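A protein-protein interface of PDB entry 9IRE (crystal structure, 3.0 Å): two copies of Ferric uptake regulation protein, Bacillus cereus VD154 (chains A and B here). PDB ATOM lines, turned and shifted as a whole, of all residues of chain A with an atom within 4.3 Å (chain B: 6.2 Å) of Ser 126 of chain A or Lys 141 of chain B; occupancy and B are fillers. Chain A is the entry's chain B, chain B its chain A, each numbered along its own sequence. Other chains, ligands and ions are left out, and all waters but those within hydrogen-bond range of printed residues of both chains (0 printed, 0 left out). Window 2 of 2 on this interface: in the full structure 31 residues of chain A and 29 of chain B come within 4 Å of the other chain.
The backbone carbonyl oxygen (O) of Ser 126 of chain A sits close to the backbone NH (N) of Lys 141 of chain B (3.3 Å).
The backbone carbonyl oxygen (O) of Ile 139 of chain B lies within hydrogen-bond range of the side-chain amide nitrogen (NE2) of Gln 144 of chain B, 3.3 Å away.
The backbone carbonyl oxygen (O) of Glu 122 of chain A sits at hydrogen-bond distance from the backbone NH (N) of Phe 127 of chain A (3.4 Å).
The side-chain sulfur (SG) of Cys 140 of chain B sits close to the backbone NH (N) of Asn 142 of chain B, at 3.8 Å.
O of Cys 140 of chain B lies within hydrogen-bond range of NE2 of Gln 144 of chain B, at 3.0 Å.
Lys 141 of chain B touches Trp 125 of chain A (CB to O, 3.8 Å).
Ser 126 of chain A touches Gln 144 of chain B (O to NE2, 3.5 Å).
CE1 of Phe 127 of chain A touches CB of Cys 140 of chain B (3.5 Å).
Of chain B, only Lys 141 and Gln 144 come within 4 Å of Ser 126 of chain A.
Lys 141 of chain B touches just these residues of chain A: Trp 125 and Ser 126.
Of the printed residues of chain A, Cys 140 of chain B touches Phe 127 (3.5 Å).
Of the printed residues of chain B, Trp 125 of chain A touches Lys 141 (3.8 Å).
Printed residues of chain A within 4 Å of Gln 144 of chain B: Ser 126 (3.5 Å).
Of the printed residues of chain B, Phe 127 of chain A touches Cys 140.
The nearest residue of chain B that does not touch Ser 126 of chain A is Cys 140 of chain B (4.2 Å).
The nearest printed residue of chain A that does not touch Lys 141 of chain B is Phe 127 of chain A (4.4 Å).
Hydrophobic or aromatic side chains of chain A that line the printed part of chain B: Phe 127.
Along chain B the printed residues that touch a printed residue of chain A span positions 140 to 144.
Among the printed residues, 4 pairs touch across the chains.
Among the printed residues, no Asp or Glu carboxylate lies within 4 Å of a Lys or Arg side-chain nitrogen of the other chain.
No position is printed for both chains.
Of the 4 pairs that touch across the chains among the printed residues, none has its exchanged pair printed and touching as well.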
ATOM      1  N   VAL A 121     -26.210  10.697   2.493  1.00  0.00           N
ATOM      2  CA  VAL A 121     -25.401   9.910   1.572  1.00  0.00           C
ATOM      3  C   VAL A 121     -25.115   8.578   2.232  1.00  0.00           C
ATOM      4  O   VAL A 121     -25.531   7.536   1.713  1.00  0.00           O
ATOM      5  CB  VAL A 121     -24.096  10.630   1.182  1.00  0.00           C
ATOM      6  CG1 VAL A 121     -23.064   9.655   0.620  1.00  0.00           C
ATOM      7  CG2 VAL A 121     -24.407  11.718   0.156  1.00  0.00           C
ATOM      8  N   GLU A 122     -24.479   8.623   3.412  1.00  0.00           N
ATOM      9  CA  GLU A 122     -24.045   7.412   4.094  1.00  0.00           C
ATOM     10  C   GLU A 122     -25.165   6.396   4.102  1.00  0.00           C
ATOM     11  O   GLU A 122     -25.038   5.343   3.476  1.00  0.00           O
ATOM     12  CB  GLU A 122     -23.563   7.728   5.510  1.00  0.00           C
ATOM     13  CG  GLU A 122     -22.219   8.443   5.489  1.00  0.00           C
ATOM     14  CD  GLU A 122     -21.646   8.726   6.864  1.00  0.00           C
ATOM     15  OE1 GLU A 122     -22.427   8.797   7.847  1.00  0.00           O
ATOM     16  OE2 GLU A 122     -20.407   8.881   6.947  1.00  0.00           O
ATOM     17  N   HIS A 123     -26.304   6.747   4.714  1.00  0.00           N
ATOM     18  CA  HIS A 123     -27.495   5.892   4.699  1.00  0.00           C
ATOM     19  C   HIS A 123     -27.866   5.429   3.297  1.00  0.00           C
ATOM     20  O   HIS A 123     -28.183   4.256   3.081  1.00  0.00           O
ATOM     21  CB  HIS A 123     -28.675   6.658   5.264  1.00  0.00           C
ATOM     22  CG  HIS A 123     -29.901   5.817   5.471  1.00  0.00           C
ATOM     23  ND1 HIS A 123     -31.174   6.350   5.465  1.00  0.00           N
ATOM     24  CD2 HIS A 123     -30.047   4.498   5.748  1.00  0.00           C
ATOM     25  CE1 HIS A 123     -32.051   5.395   5.719  1.00  0.00           C
ATOM     26  NE2 HIS A 123     -31.396   4.260   5.892  1.00  0.00           N
ATOM     27  N   ASP A 124     -27.882   6.364   2.333  1.00  0.00           N
ATOM     28  CA  ASP A 124     -28.506   6.109   1.037  1.00  0.00           C
ATOM     29  C   ASP A 124     -27.654   5.217   0.150  1.00  0.00           C
ATOM     30  O   ASP A 124     -28.193   4.520  -0.721  1.00  0.00           O
ATOM     31  CB  ASP A 124     -28.799   7.439   0.338  1.00  0.00           C
ATOM     32  CG  ASP A 124     -30.212   7.991   0.673  1.00  0.00           C
ATOM     33  OD1 ASP A 124     -30.747   7.614   1.750  1.00  0.00           O
ATOM     34  OD2 ASP A 124     -30.805   8.767  -0.136  1.00  0.00           O
ATOM     35  N   TRP A 125     -26.324   5.248   0.348  1.00  0.00           N
ATOM     36  CA  TRP A 125     -25.317   4.577  -0.473  1.00  0.00           C
ATOM     37  C   TRP A 125     -24.440   3.605   0.320  1.00  0.00           C
ATOM     38  O   TRP A 125     -23.642   2.861  -0.280  1.00  0.00           O
ATOM     39  CB  TRP A 125     -24.446   5.647  -1.160  1.00  0.00           C
ATOM     40  CG  TRP A 125     -25.203   6.308  -2.286  1.00  0.00           C
ATOM     41  CD1 TRP A 125     -25.995   7.450  -2.223  1.00  0.00           C
ATOM     42  CD2 TRP A 125     -25.295   5.836  -3.639  1.00  0.00           C
ATOM     43  NE1 TRP A 125     -26.548   7.706  -3.461  1.00  0.00           N
ATOM     44  CE2 TRP A 125     -26.127   6.734  -4.346  1.00  0.00           C
ATOM     45  CE3 TRP A 125     -24.726   4.754  -4.334  1.00  0.00           C
ATOM     46  CZ2 TRP A 125     -26.404   6.559  -5.726  1.00  0.00           C
ATOM     47  CZ3 TRP A 125     -24.987   4.604  -5.695  1.00  0.00           C
ATOM     48  CH2 TRP A 125     -25.819   5.492  -6.370  1.00  0.00           C
ATOM     49  N   SER A 126     -24.589   3.566   1.642  1.00  0.00           N
ATOM     50  CA  SER A 126     -23.729   2.795   2.531  1.00  0.00           C
ATOM     51  C   SER A 126     -22.286   3.120   2.222  1.00  0.00           C
ATOM     52  O   SER A 126     -21.516   2.302   1.741  1.00  0.00           O
ATOM     53  CB  SER A 126     -24.034   1.311   2.429  1.00  0.00           C
ATOM     54  OG  SER A 126     -25.340   1.095   2.948  1.00  0.00           O
ATOM     55  N   PHE A 127     -21.983   4.393   2.410  1.00  0.00           N
ATOM     56  CA  PHE A 127     -20.685   4.968   2.130  1.00  0.00           C
ATOM     57  C   PHE A 127     -20.172   5.562   3.423  1.00  0.00           C
ATOM     58  O   PHE A 127     -20.935   6.124   4.212  1.00  0.00           O
ATOM     59  CB  PHE A 127     -20.821   6.035   1.060  1.00  0.00           C
ATOM     60  CG  PHE A 127     -19.573   6.328   0.304  1.00  0.00           C
ATOM     61  CD1 PHE A 127     -19.168   5.518  -0.729  1.00  0.00           C
ATOM     62  CD2 PHE A 127     -18.826   7.456   0.584  1.00  0.00           C
ATOM     63  CE1 PHE A 127     -18.018   5.818  -1.447  1.00  0.00           C
ATOM     64  CE2 PHE A 127     -17.690   7.749  -0.140  1.00  0.00           C
ATOM     65  CZ  PHE A 127     -17.291   6.937  -1.147  1.00  0.00           C
ATOM     66  N   CYS B 100     -14.064   6.470  -4.019  1.00  0.00           N
ATOM     67  CA  CYS B 100     -13.489   5.578  -3.028  1.00  0.00           C
ATOM     68  C   CYS B 100     -11.979   5.777  -3.000  1.00  0.00           C
ATOM     69  O   CYS B 100     -11.331   5.837  -4.047  1.00  0.00           O
ATOM     70  CB  CYS B 100     -13.832   4.133  -3.365  1.00  0.00           C
ATOM     71  SG  CYS B 100     -13.445   3.037  -2.045  1.00  0.00           S
ATOM     72  N   ILE B 139     -13.991   5.349   2.129  1.00  0.00           N
ATOM     73  CA  ILE B 139     -13.915   3.959   1.712  1.00  0.00           C
ATOM     74  C   ILE B 139     -15.347   3.452   1.532  1.00  0.00           C
ATOM     75  O   ILE B 139     -16.217   3.676   2.391  1.00  0.00           O
ATOM     76  CB  ILE B 139     -13.045   3.163   2.704  1.00  0.00           C
ATOM     77  CG1 ILE B 139     -11.547   3.371   2.346  1.00  0.00           C
ATOM     78  CG2 ILE B 139     -13.431   1.701   2.755  1.00  0.00           C
ATOM     79  CD1 ILE B 139     -10.467   2.764   3.305  1.00  0.00           C
ATOM     80  N   CYS B 140     -15.618   2.858   0.363  1.00  0.00           N
ATOM     81  CA  CYS B 140     -16.989   2.637  -0.100  1.00  0.00           C
ATOM     82  C   CYS B 140     -17.643   1.389   0.522  1.00  0.00           C
ATOM     83  O   CYS B 140     -17.048   0.644   1.309  1.00  0.00           O
ATOM     84  CB  CYS B 140     -17.021   2.518  -1.618  1.00  0.00           C
ATOM     85  SG  CYS B 140     -16.429   0.899  -2.164  1.00  0.00           S
ATOM     86  N   LYS B 141     -18.896   1.163   0.116  1.00  0.00           N
ATOM     87  CA  LYS B 141     -19.736   0.164   0.766  1.00  0.00           C
ATOM     88  C   LYS B 141     -19.064  -1.184   0.806  1.00  0.00           C
ATOM     89  O   LYS B 141     -19.004  -1.828   1.858  1.00  0.00           O
ATOM     90  CB  LYS B 141     -21.078   0.019   0.043  1.00  0.00           C
ATOM     91  CG  LYS B 141     -21.892  -1.163   0.575  1.00  0.00           C
ATOM     92  CD  LYS B 141     -23.258  -1.213  -0.039  1.00  0.00           C
ATOM     93  CE  LYS B 141     -24.052  -2.355   0.537  1.00  0.00           C
ATOM     94  NZ  LYS B 141     -25.522  -2.223   0.230  1.00  0.00           N
ATOM     95  N   ASN B 142     -18.586  -1.637  -0.352  1.00  0.00           N
ATOM     96  CA  ASN B 142     -18.004  -2.966  -0.480  1.00  0.00           C
ATOM     97  C   ASN B 142     -16.597  -3.063   0.110  1.00  0.00           C
ATOM     98  O   ASN B 142     -16.161  -4.177   0.427  1.00  0.00           O
ATOM     99  CB  ASN B 142     -17.974  -3.379  -1.956  1.00  0.00           C
ATOM    100  CG  ASN B 142     -19.202  -4.128  -2.384  1.00  0.00           C
ATOM    101  OD1 ASN B 142     -19.901  -3.710  -3.301  1.00  0.00           O
ATOM    102  ND2 ASN B 142     -19.471  -5.254  -1.735  1.00  0.00           N
ATOM    103  N   CYS B 143     -15.878  -1.941   0.265  1.00  0.00           N
ATOM    104  CA  CYS B 143     -14.603  -1.997   0.956  1.00  0.00           C
ATOM    105  C   CYS B 143     -14.759  -2.004   2.461  1.00  0.00           C
ATOM    106  O   CYS B 143     -13.769  -2.185   3.170  1.00  0.00           O
ATOM    107  CB  CYS B 143     -13.714  -0.832   0.564  1.00  0.00           C
ATOM    108  SG  CYS B 143     -13.348  -0.831  -1.164  1.00  0.00           S
ATOM    109  N   GLN B 144     -15.964  -1.795   2.970  1.00  0.00           N
ATOM    110  CA  GLN B 144     -16.195  -2.036   4.385  1.00  0.00           C
ATOM    111  C   GLN B 144     -16.288  -3.521   4.671  1.00  0.00           C
ATOM    112  O   GLN B 144     -15.875  -3.967   5.752  1.00  0.00           O
ATOM    113  CB  GLN B 144     -17.449  -1.286   4.836  1.00  0.00           C
ATOM    114  CG  GLN B 144     -17.201   0.214   4.831  1.00  0.00           C
ATOM    115  CD  GLN B 144     -18.456   1.038   4.727  1.00  0.00           C
ATOM    116  OE1 GLN B 144     -19.293   1.066   5.645  1.00  0.00           O
ATOM    117  NE2 GLN B 144     -18.593   1.743   3.612  1.00  0.00           N
ATOM    118  N   GLU B 145     -16.757  -4.297   3.691  1.00  0.00           N
ATOM    119  CA  GLU B 145     -17.105  -5.700   3.871  1.00  0.00           C
ATOM    120  C   GLU B 145     -16.129  -6.663   3.204  1.00  0.00           C
ATOM    121  O   GLU B 145     -16.363  -7.880   3.224  1.00  0.00           O
ATOM    122  CB  GLU B 145     -18.536  -5.923   3.360  1.00  0.00           C
ATOM    123  CG  GLU B 145     -19.539  -5.000   4.078  1.00  0.00           C
ATOM    124  CD  GLU B 145     -20.637  -4.464   3.176  1.00  0.00           C
ATOM    125  OE1 GLU B 145     -20.438  -4.470   1.946  1.00  0.00           O
ATOM    126  OE2 GLU B 145     -21.696  -4.037   3.708  1.00  0.00           O
ATOM    127  N   ASN B 146     -15.041  -6.151   2.618  1.00  0.00           N
ATOM    128  CA  ASN B 146     -13.949  -6.971   2.118  1.00  0.00           C
ATOM    129  C   ASN B 146     -12.640  -6.703   2.837  1.00  0.00           C
ATOM    130  O   ASN B 146     -11.651  -7.395   2.568  1.00  0.00           O
ATOM    131  CB  ASN B 146     -13.774  -6.764   0.612  1.00  0.00           C
ATOM    132  CG  ASN B 146     -14.963  -7.269  -0.166  1.00  0.00           C
ATOM    133  OD1 ASN B 146     -15.749  -8.073   0.343  1.00  0.00           O
ATOM    134  ND2 ASN B 146     -15.108  -6.811  -1.400  1.00  0.00           N
